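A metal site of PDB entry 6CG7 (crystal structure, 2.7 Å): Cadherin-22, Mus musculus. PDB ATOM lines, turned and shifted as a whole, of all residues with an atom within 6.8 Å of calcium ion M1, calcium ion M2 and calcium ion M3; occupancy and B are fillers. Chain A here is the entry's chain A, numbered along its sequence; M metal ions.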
ATOM      1  N   GLU A  11     -33.814  -3.594   1.119  1.00  0.00           N
ATOM      2  CA  GLU A  11     -33.372  -2.720   0.057  1.00  0.00           C
ATOM      3  C   GLU A  11     -34.273  -2.869  -1.178  1.00  0.00           C
ATOM      4  O   GLU A  11     -35.099  -3.780  -1.272  1.00  0.00           O
ATOM      5  CB  GLU A  11     -31.919  -3.011  -0.345  1.00  0.00           C
ATOM      6  CG  GLU A  11     -31.703  -4.378  -0.984  1.00  0.00           C
ATOM      7  CD  GLU A  11     -30.352  -4.478  -1.686  1.00  0.00           C
ATOM      8  OE1 GLU A  11     -29.736  -5.567  -1.650  1.00  0.00           O
ATOM      9  OE2 GLU A  11     -29.917  -3.468  -2.281  1.00  0.00           O
ATOM     10  N   GLU A  12     -34.087  -1.947  -2.114  1.00  0.00           N
ATOM     11  CA  GLU A  12     -34.758  -1.972  -3.406  1.00  0.00           C
ATOM     12  C   GLU A  12     -36.266  -2.179  -3.259  1.00  0.00           C
ATOM     13  O   GLU A  12     -36.879  -2.975  -3.961  1.00  0.00           O
ATOM     14  CB  GLU A  12     -34.156  -3.050  -4.314  1.00  0.00           C
ATOM     15  CG  GLU A  12     -32.641  -3.119  -4.319  1.00  0.00           C
ATOM     16  CD  GLU A  12     -31.996  -1.879  -4.915  1.00  0.00           C
ATOM     17  OE1 GLU A  12     -32.695  -1.136  -5.631  1.00  0.00           O
ATOM     18  OE2 GLU A  12     -30.794  -1.639  -4.654  1.00  0.00           O
ATOM     19  N   LEU A  63     -33.972   2.123  -1.078  1.00  0.00           N
ATOM     20  CA  LEU A  63     -32.639   1.999  -0.500  1.00  0.00           C
ATOM     21  C   LEU A  63     -31.826   0.961  -1.279  1.00  0.00           C
ATOM     22  O   LEU A  63     -32.377   0.010  -1.837  1.00  0.00           O
ATOM     23  CB  LEU A  63     -32.721   1.602   0.969  1.00  0.00           C
ATOM     24  CG  LEU A  63     -33.425   2.588   1.907  1.00  0.00           C
ATOM     25  CD1 LEU A  63     -33.571   1.980   3.298  1.00  0.00           C
ATOM     26  CD2 LEU A  63     -32.690   3.909   1.982  1.00  0.00           C
ATOM     27  N   ASP A  64     -30.511   1.159  -1.293  1.00  0.00           N
ATOM     28  CA  ASP A  64     -29.585   0.296  -2.021  1.00  0.00           C
ATOM     29  C   ASP A  64     -28.455  -0.113  -1.086  1.00  0.00           C
ATOM     30  O   ASP A  64     -27.645   0.722  -0.695  1.00  0.00           O
ATOM     31  CB  ASP A  64     -29.047   1.002  -3.260  1.00  0.00           C
ATOM     32  CG  ASP A  64     -28.117   0.132  -4.086  1.00  0.00           C
ATOM     33  OD1 ASP A  64     -28.173  -1.108  -3.935  1.00  0.00           O
ATOM     34  OD2 ASP A  64     -27.341   0.683  -4.889  1.00  0.00           O
ATOM     35  N   ARG A  65     -28.404  -1.408  -0.736  1.00  0.00           N
ATOM     36  CA  ARG A  65     -27.367  -1.879   0.169  1.00  0.00           C
ATOM     37  C   ARG A  65     -25.993  -1.813  -0.474  1.00  0.00           C
ATOM     38  O   ARG A  65     -24.991  -1.532   0.196  1.00  0.00           O
ATOM     39  CB  ARG A  65     -27.668  -3.310   0.609  1.00  0.00           C
ATOM     40  CG  ARG A  65     -26.880  -3.770   1.820  1.00  0.00           C
ATOM     41  CD  ARG A  65     -26.860  -5.286   1.941  1.00  0.00           C
ATOM     42  NE  ARG A  65     -26.107  -5.889   0.846  1.00  0.00           N
ATOM     43  CZ  ARG A  65     -24.782  -5.959   0.805  1.00  0.00           C
ATOM     44  NH1 ARG A  65     -24.049  -5.462   1.807  1.00  0.00           N
ATOM     45  NH2 ARG A  65     -24.173  -6.525  -0.229  1.00  0.00           N
ATOM     46  N   GLU A  66     -25.924  -2.061  -1.787  1.00  0.00           N
ATOM     47  CA  GLU A  66     -24.663  -1.951  -2.506  1.00  0.00           C
ATOM     48  C   GLU A  66     -24.170  -0.519  -2.601  1.00  0.00           C
ATOM     49  O   GLU A  66     -23.025  -0.298  -2.989  1.00  0.00           O
ATOM     50  CB  GLU A  66     -24.790  -2.566  -3.905  1.00  0.00           C
ATOM     51  CG  GLU A  66     -24.855  -4.089  -3.923  1.00  0.00           C
ATOM     52  CD  GLU A  66     -26.132  -4.641  -3.312  1.00  0.00           C
ATOM     53  OE1 GLU A  66     -27.213  -4.059  -3.555  1.00  0.00           O
ATOM     54  OE2 GLU A  66     -26.058  -5.655  -2.593  1.00  0.00           O
ATOM     55  N   GLN A  67     -25.017   0.461  -2.282  1.00  0.00           N
ATOM     56  CA  GLN A  67     -24.603   1.854  -2.167  1.00  0.00           C
ATOM     57  C   GLN A  67     -24.249   2.208  -0.734  1.00  0.00           C
ATOM     58  O   GLN A  67     -23.197   2.795  -0.477  1.00  0.00           O
ATOM     59  CB  GLN A  67     -25.715   2.777  -2.684  1.00  0.00           C
ATOM     60  CG  GLN A  67     -25.363   4.263  -2.672  1.00  0.00           C
ATOM     61  CD  GLN A  67     -26.557   5.151  -2.355  1.00  0.00           C
ATOM     62  OE1 GLN A  67     -27.633   4.669  -1.993  1.00  0.00           O
ATOM     63  NE2 GLN A  67     -26.363   6.460  -2.482  1.00  0.00           N
ATOM     64  N   GLN A  97     -31.263  -4.411   4.672  1.00  0.00           N
ATOM     65  CA  GLN A  97     -30.989  -5.813   4.435  1.00  0.00           C
ATOM     66  C   GLN A  97     -30.812  -6.095   2.946  1.00  0.00           C
ATOM     67  O   GLN A  97     -31.283  -5.349   2.078  1.00  0.00           O
ATOM     68  CB  GLN A  97     -32.107  -6.688   5.014  1.00  0.00           C
ATOM     69  CG  GLN A  97     -31.822  -8.198   4.987  1.00  0.00           C
ATOM     70  CD  GLN A  97     -30.533  -8.571   5.710  1.00  0.00           C
ATOM     71  OE1 GLN A  97     -29.586  -9.063   5.104  1.00  0.00           O
ATOM     72  NE2 GLN A  97     -30.508  -8.342   7.013  1.00  0.00           N
ATOM     73  N   ASP A  98     -30.123  -7.196   2.648  1.00  0.00           N
ATOM     74  CA  ASP A  98     -29.708  -7.540   1.306  1.00  0.00           C
ATOM     75  C   ASP A  98     -30.784  -8.331   0.567  1.00  0.00           C
ATOM     76  O   ASP A  98     -31.518  -9.116   1.175  1.00  0.00           O
ATOM     77  CB  ASP A  98     -28.416  -8.370   1.352  1.00  0.00           C
ATOM     78  CG  ASP A  98     -27.959  -8.827  -0.004  1.00  0.00           C
ATOM     79  OD1 ASP A  98     -27.568  -7.957  -0.815  1.00  0.00           O
ATOM     80  OD2 ASP A  98     -27.988 -10.044  -0.267  1.00  0.00           O
ATOM     81  N   ILE A  99     -30.871  -8.094  -0.739  1.00  0.00           N
ATOM     82  CA  ILE A  99     -31.634  -8.951  -1.642  1.00  0.00           C
ATOM     83  C   ILE A  99     -30.715  -9.316  -2.801  1.00  0.00           C
ATOM     84  O   ILE A  99     -29.753  -8.617  -3.120  1.00  0.00           O
ATOM     85  CB  ILE A  99     -32.922  -8.278  -2.176  1.00  0.00           C
ATOM     86  CG1 ILE A  99     -32.594  -7.140  -3.147  1.00  0.00           C
ATOM     87  CG2 ILE A  99     -33.780  -7.785  -1.009  1.00  0.00           C
ATOM     88  CD1 ILE A  99     -33.787  -6.533  -3.827  1.00  0.00           C
ATOM     89  N   ASN A 100     -31.019 -10.446  -3.440  1.00  0.00           N
ATOM     90  CA  ASN A 100     -30.217 -10.944  -4.561  1.00  0.00           C
ATOM     91  C   ASN A 100     -30.566 -10.134  -5.805  1.00  0.00           C
ATOM     92  O   ASN A 100     -31.374 -10.538  -6.655  1.00  0.00           O
ATOM     93  CB  ASN A 100     -30.445 -12.424  -4.773  1.00  0.00           C
ATOM     94  CG  ASN A 100     -29.551 -13.001  -5.846  1.00  0.00           C
ATOM     95  OD1 ASN A 100     -28.483 -12.463  -6.132  1.00  0.00           O
ATOM     96  ND2 ASN A 100     -29.987 -14.099  -6.464  1.00  0.00           N
ATOM     97  N   ASP A 101     -29.924  -8.966  -5.927  1.00  0.00           N
ATOM     98  CA  ASP A 101     -30.133  -8.088  -7.078  1.00  0.00           C
ATOM     99  C   ASP A 101     -28.815  -7.710  -7.750  1.00  0.00           C
ATOM    100  O   ASP A 101     -28.758  -6.697  -8.459  1.00  0.00           O
ATOM    101  CB  ASP A 101     -30.899  -6.833  -6.669  1.00  0.00           C
ATOM    102  CG  ASP A 101     -30.098  -5.949  -5.723  1.00  0.00           C
ATOM    103  OD1 ASP A 101     -30.182  -4.712  -5.856  1.00  0.00           O
ATOM    104  OD2 ASP A 101     -29.398  -6.495  -4.848  1.00  0.00           O
ATOM    105  N   SER A 102     -27.758  -8.493  -7.557  1.00  0.00           N
ATOM    106  CA  SER A 102     -26.466  -8.258  -8.191  1.00  0.00           C
ATOM    107  C   SER A 102     -26.050  -9.509  -8.943  1.00  0.00           C
ATOM    108  O   SER A 102     -25.911 -10.576  -8.345  1.00  0.00           O
ATOM    109  CB  SER A 102     -25.409  -7.878  -7.143  1.00  0.00           C
ATOM    110  OG  SER A 102     -25.824  -6.776  -6.366  1.00  0.00           O
ATOM    111  N   GLU A 103     -25.850  -9.381 -10.255  1.00  0.00           N
ATOM    112  CA  GLU A 103     -25.421 -10.508 -11.064  1.00  0.00           C
ATOM    113  C   GLU A 103     -23.953 -10.850 -10.770  1.00  0.00           C
ATOM    114  O   GLU A 103     -23.161  -9.961 -10.451  1.00  0.00           O
ATOM    115  CB  GLU A 103     -25.580 -10.212 -12.548  1.00  0.00           C
ATOM    116  CG  GLU A 103     -27.009 -10.148 -13.052  1.00  0.00           C
ATOM    117  CD  GLU A 103     -27.105 -10.296 -14.558  1.00  0.00           C
ATOM    118  OE1 GLU A 103     -26.058 -10.526 -15.211  1.00  0.00           O
ATOM    119  OE2 GLU A 103     -28.225 -10.188 -15.096  1.00  0.00           O
ATOM    120  N   PRO A 104     -23.577 -12.126 -10.871  1.00  0.00           N
ATOM    121  CA  PRO A 104     -22.154 -12.458 -10.818  1.00  0.00           C
ATOM    122  C   PRO A 104     -21.421 -11.888 -12.014  1.00  0.00           C
ATOM    123  O   PRO A 104     -21.945 -11.861 -13.129  1.00  0.00           O
ATOM    124  CB  PRO A 104     -22.136 -13.997 -10.824  1.00  0.00           C
ATOM    125  CG  PRO A 104     -23.507 -14.396 -10.420  1.00  0.00           C
ATOM    126  CD  PRO A 104     -24.416 -13.334 -10.940  1.00  0.00           C
ATOM    127  N   ASP A 132     -19.677 -11.412  -6.639  1.00  0.00           N
ATOM    128  CA  ASP A 132     -21.090 -11.078  -6.458  1.00  0.00           C
ATOM    129  C   ASP A 132     -21.183  -9.989  -5.410  1.00  0.00           C
ATOM    130  O   ASP A 132     -20.740 -10.175  -4.268  1.00  0.00           O
ATOM    131  CB  ASP A 132     -21.892 -12.311  -6.035  1.00  0.00           C
ATOM    132  CG  ASP A 132     -23.380 -12.139  -6.229  1.00  0.00           C
ATOM    133  OD1 ASP A 132     -23.986 -12.971  -6.927  1.00  0.00           O
ATOM    134  OD2 ASP A 132     -23.949 -11.170  -5.681  1.00  0.00           O
ATOM    135  N   ALA A 133     -21.754  -8.845  -5.790  1.00  0.00           N
ATOM    136  CA  ALA A 133     -21.793  -7.689  -4.899  1.00  0.00           C
ATOM    137  C   ALA A 133     -22.800  -7.844  -3.769  1.00  0.00           C
ATOM    138  O   ALA A 133     -22.866  -6.958  -2.910  1.00  0.00           O
ATOM    139  CB  ALA A 133     -22.122  -6.427  -5.703  1.00  0.00           C
ATOM    140  N   ASP A 134     -23.580  -8.923  -3.743  1.00  0.00           N
ATOM    141  CA  ASP A 134     -24.571  -9.115  -2.701  1.00  0.00           C
ATOM    142  C   ASP A 134     -23.887  -9.534  -1.396  1.00  0.00           C
ATOM    143  O   ASP A 134     -22.665  -9.659  -1.311  1.00  0.00           O
ATOM    144  CB  ASP A 134     -25.611 -10.139  -3.145  1.00  0.00           C
ATOM    145  CG  ASP A 134     -26.468  -9.638  -4.305  1.00  0.00           C
ATOM    146  OD1 ASP A 134     -26.730  -8.416  -4.360  1.00  0.00           O
ATOM    147  OD2 ASP A 134     -26.873 -10.456  -5.148  1.00  0.00           O
ATOM    148  N   ASP A 135     -24.695  -9.771  -0.362  1.00  0.00           N
ATOM    149  CA  ASP A 135     -24.191 -10.101   0.965  1.00  0.00           C
ATOM    150  C   ASP A 135     -23.795 -11.567   1.047  1.00  0.00           C
ATOM    151  O   ASP A 135     -24.672 -12.449   0.956  1.00  0.00           O
ATOM    152  CB  ASP A 135     -25.243  -9.783   2.035  1.00  0.00           C
ATOM    153  CG  ASP A 135     -24.667  -9.795   3.442  1.00  0.00           C
ATOM    154  OD1 ASP A 135     -25.220  -9.110   4.327  1.00  0.00           O
ATOM    155  OD2 ASP A 135     -23.635 -10.473   3.663  1.00  0.00           O
ATOM    156  N   SER A 140     -27.872 -17.286   0.261  1.00  0.00           N
ATOM    157  CA  SER A 140     -27.048 -17.708  -0.864  1.00  0.00           C
ATOM    158  C   SER A 140     -26.987 -16.661  -1.966  1.00  0.00           C
ATOM    159  O   SER A 140     -26.672 -16.991  -3.112  1.00  0.00           O
ATOM    160  CB  SER A 140     -27.572 -19.041  -1.425  1.00  0.00           C
ATOM    161  OG  SER A 140     -27.543 -20.059  -0.442  1.00  0.00           O
ATOM    162  N   SER A 141     -27.277 -15.399  -1.631  1.00  0.00           N
ATOM    163  CA  SER A 141     -27.290 -14.343  -2.639  1.00  0.00           C
ATOM    164  C   SER A 141     -25.929 -14.155  -3.300  1.00  0.00           C
ATOM    165  O   SER A 141     -25.859 -13.609  -4.403  1.00  0.00           O
ATOM    166  CB  SER A 141     -27.743 -13.017  -2.003  1.00  0.00           C
ATOM    167  OG  SER A 141     -29.026 -13.136  -1.431  1.00  0.00           O
ATOM    168  N   ALA A 142     -24.846 -14.592  -2.644  1.00  0.00           N
ATOM    169  CA  ALA A 142     -23.511 -14.457  -3.187  1.00  0.00           C
ATOM    170  C   ALA A 142     -22.755 -15.778  -3.247  1.00  0.00           C
ATOM    171  O   ALA A 142     -21.540 -15.774  -3.454  1.00  0.00           O
ATOM    172  CB  ALA A 142     -22.704 -13.434  -2.381  1.00  0.00           C
ATOM    173  N   ARG A 143     -23.437 -16.906  -3.040  1.00  0.00           N
ATOM    174  CA  ARG A 143     -22.818 -18.221  -3.147  1.00  0.00           C
ATOM    175  C   ARG A 143     -22.986 -18.719  -4.573  1.00  0.00           C
ATOM    176  O   ARG A 143     -24.106 -18.989  -5.013  1.00  0.00           O
ATOM    177  CB  ARG A 143     -23.424 -19.192  -2.127  1.00  0.00           C
ATOM    178  CG  ARG A 143     -23.073 -18.831  -0.700  1.00  0.00           C
ATOM    179  CD  ARG A 143     -23.668 -19.789   0.315  1.00  0.00           C
ATOM    180  NE  ARG A 143     -23.463 -19.293   1.681  1.00  0.00           N
ATOM    181  CZ  ARG A 143     -23.953 -19.866   2.774  1.00  0.00           C
ATOM    182  NH1 ARG A 143     -24.686 -20.974   2.680  1.00  0.00           N
ATOM    183  NH2 ARG A 143     -23.708 -19.337   3.968  1.00  0.00           N
ATOM    184  N   LEU A 144     -21.882 -18.833  -5.305  1.00  0.00           N
ATOM    185  CA  LEU A 144     -21.902 -19.028  -6.739  1.00  0.00           C
ATOM    186  C   LEU A 144     -21.651 -20.495  -7.107  1.00  0.00           C
ATOM    187  O   LEU A 144     -21.082 -21.267  -6.346  1.00  0.00           O
ATOM    188  CB  LEU A 144     -20.841 -18.146  -7.407  1.00  0.00           C
ATOM    189  CG  LEU A 144     -20.925 -16.652  -7.055  1.00  0.00           C
ATOM    190  CD1 LEU A 144     -19.788 -15.893  -7.714  1.00  0.00           C
ATOM    191  CD2 LEU A 144     -22.267 -16.062  -7.448  1.00  0.00           C
ATOM    192  N   ASP A 187     -25.530 -17.521  -8.949  1.00  0.00           N
ATOM    193  CA  ASP A 187     -25.689 -17.416  -7.500  1.00  0.00           C
ATOM    194  C   ASP A 187     -26.885 -18.247  -7.041  1.00  0.00           C
ATOM    195  O   ASP A 187     -27.403 -19.094  -7.785  1.00  0.00           O
ATOM    196  CB  ASP A 187     -25.793 -15.937  -7.097  1.00  0.00           C
ATOM    197  CG  ASP A 187     -26.961 -15.231  -7.759  1.00  0.00           C
ATOM    198  OD1 ASP A 187     -27.952 -15.905  -8.111  1.00  0.00           O
ATOM    199  OD2 ASP A 187     -26.883 -13.988  -7.913  1.00  0.00           O
ATOM    200  N   MET A 188     -27.343 -18.013  -5.811  1.00  0.00           N
ATOM    201  CA  MET A 188     -28.381 -18.830  -5.187  1.00  0.00           C
ATOM    202  C   MET A 188     -28.029 -20.309  -5.162  1.00  0.00           C
ATOM    203  O   MET A 188     -28.917 -21.163  -5.088  1.00  0.00           O
ATOM    204  CB  MET A 188     -29.739 -18.625  -5.881  1.00  0.00           C
ATOM    205  CG  MET A 188     -30.294 -17.220  -5.791  1.00  0.00           C
ATOM    206  SD  MET A 188     -30.634 -16.654  -4.115  1.00  0.00           S
ATOM    207  CE  MET A 188     -31.851 -17.862  -3.578  1.00  0.00           C
ATOM    208  N   LEU A 195     -29.285 -15.433 -10.386  1.00  0.00           N
ATOM    209  CA  LEU A 195     -28.702 -14.588 -11.410  1.00  0.00           C
ATOM    210  C   LEU A 195     -27.409 -15.211 -11.949  1.00  0.00           C
ATOM    211  O   LEU A 195     -26.779 -16.049 -11.291  1.00  0.00           O
ATOM    212  CB  LEU A 195     -28.428 -13.195 -10.845  1.00  0.00           C
ATOM    213  CG  LEU A 195     -29.612 -12.536 -10.132  1.00  0.00           C
ATOM    214  CD1 LEU A 195     -29.205 -11.213  -9.509  1.00  0.00           C
ATOM    215  CD2 LEU A 195     -30.777 -12.346 -11.086  1.00  0.00           C
HETATM  216 CA    CA M   1     -28.934  -3.124  -4.670  1.00  0.00          CA
HETATM  217 CA    CA M   2     -28.015  -6.951  -2.960  1.00  0.00          CA
HETATM  218 CA    CA M   3     -26.140 -12.232  -6.479  1.00  0.00          CA
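The side-chain carboxylate (OE2) of Glu 66 lies close to the guanidinium group (NH2) of Arg 65 (3.1 Å).
N of Glu 12 lies within hydrogen-bond range of O of Leu 63 (2.6 Å).
SD of Met 188 sits close to ND2 of Asn 100.
The side-chain hydroxyl of Ser 141 sits close to the side-chain carboxylate of Asp 98 (3.5 Å).
The guanidinium group (NE) of Arg 65 sits close to the side-chain carboxylate (OD1) of Asp 98 (3.0 Å).
The side-chain carboxylate of Asp 98 is in hydrogen-bond range of the backbone NH of Asp 135 (3.3 Å).
The side-chain carboxylate (OE2) of Glu 11 lies close to the backbone NH (N) of Arg 65, at 3.0 Å.
The backbone NH of Glu 11 sits at hydrogen-bond distance from the backbone carbonyl oxygen of Gln 97, 3.2 Å away.
The nearest printed residue that does not touch calcium ion M1 is Arg 65 (4.3 Å).
Six residues have an atom within 4 Å of calcium ion M2: Glu 11, Glu 66, Asp 98, Ile 99, Asp 101 and Asp 134.
The nearest printed residue that does not touch calcium ion M2 is Ser 102 (4.1 Å).
The nearest printed residue that does not touch calcium ion M3 is Leu 195 (4.4 Å).
Calcium ion M1 is bound by OE1 of Glu 66 (2.3 Å).
Calcium ion M1 is bound by OD1 of Asp 64 (2.3 Å).
The side-chain carboxylate (OD1) of Asp 101 is bound to calcium ion M1.
Calcium ion M1 is bound by the side-chain carboxylate (OE2) of Glu 12 (2.4 Å).
Calcium ion M1 is bound by OE2 of Glu 11.
The side-chain carboxylate (OE2) of Glu 66 binds calcium ion M2.
Calcium ion M2 is bound by OD2 of Asp 101, at 2.4 Å.
Calcium ion M2 is bound by OD1 of Asp 134 (2.4 Å).
OD1 of Asp 98 is bound to calcium ion M2, at 2.4 Å.
Calcium ion M2 is bound by O of Ile 99 (2.4 Å).
OE1 of Glu 11 binds calcium ion M2.
Slightly farther from calcium ion M2 lies OE1 of Glu 66 (3.1 Å).
Calcium ion M3 is bound by the side-chain carboxylate (OD1) of Asp 132 (2.3 Å).
OD2 of Asp 134 binds calcium ion M3 (2.3 Å).
Calcium ion M3 is bound by OD1 of Asn 100, 2.4 Å away.
Calcium ion M3 is bound by OD2 of Asp 187, 2.4 Å away.
O of Ser 102 binds calcium ion M3 (2.5 Å).
O of Ser 141 binds calcium ion M3 (2.5 Å).
Calcium ion M3 is bound by the side-chain carboxylate (OD2) of Asp 132.
Calcium ion M3 has seven donor atoms within binding distance.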
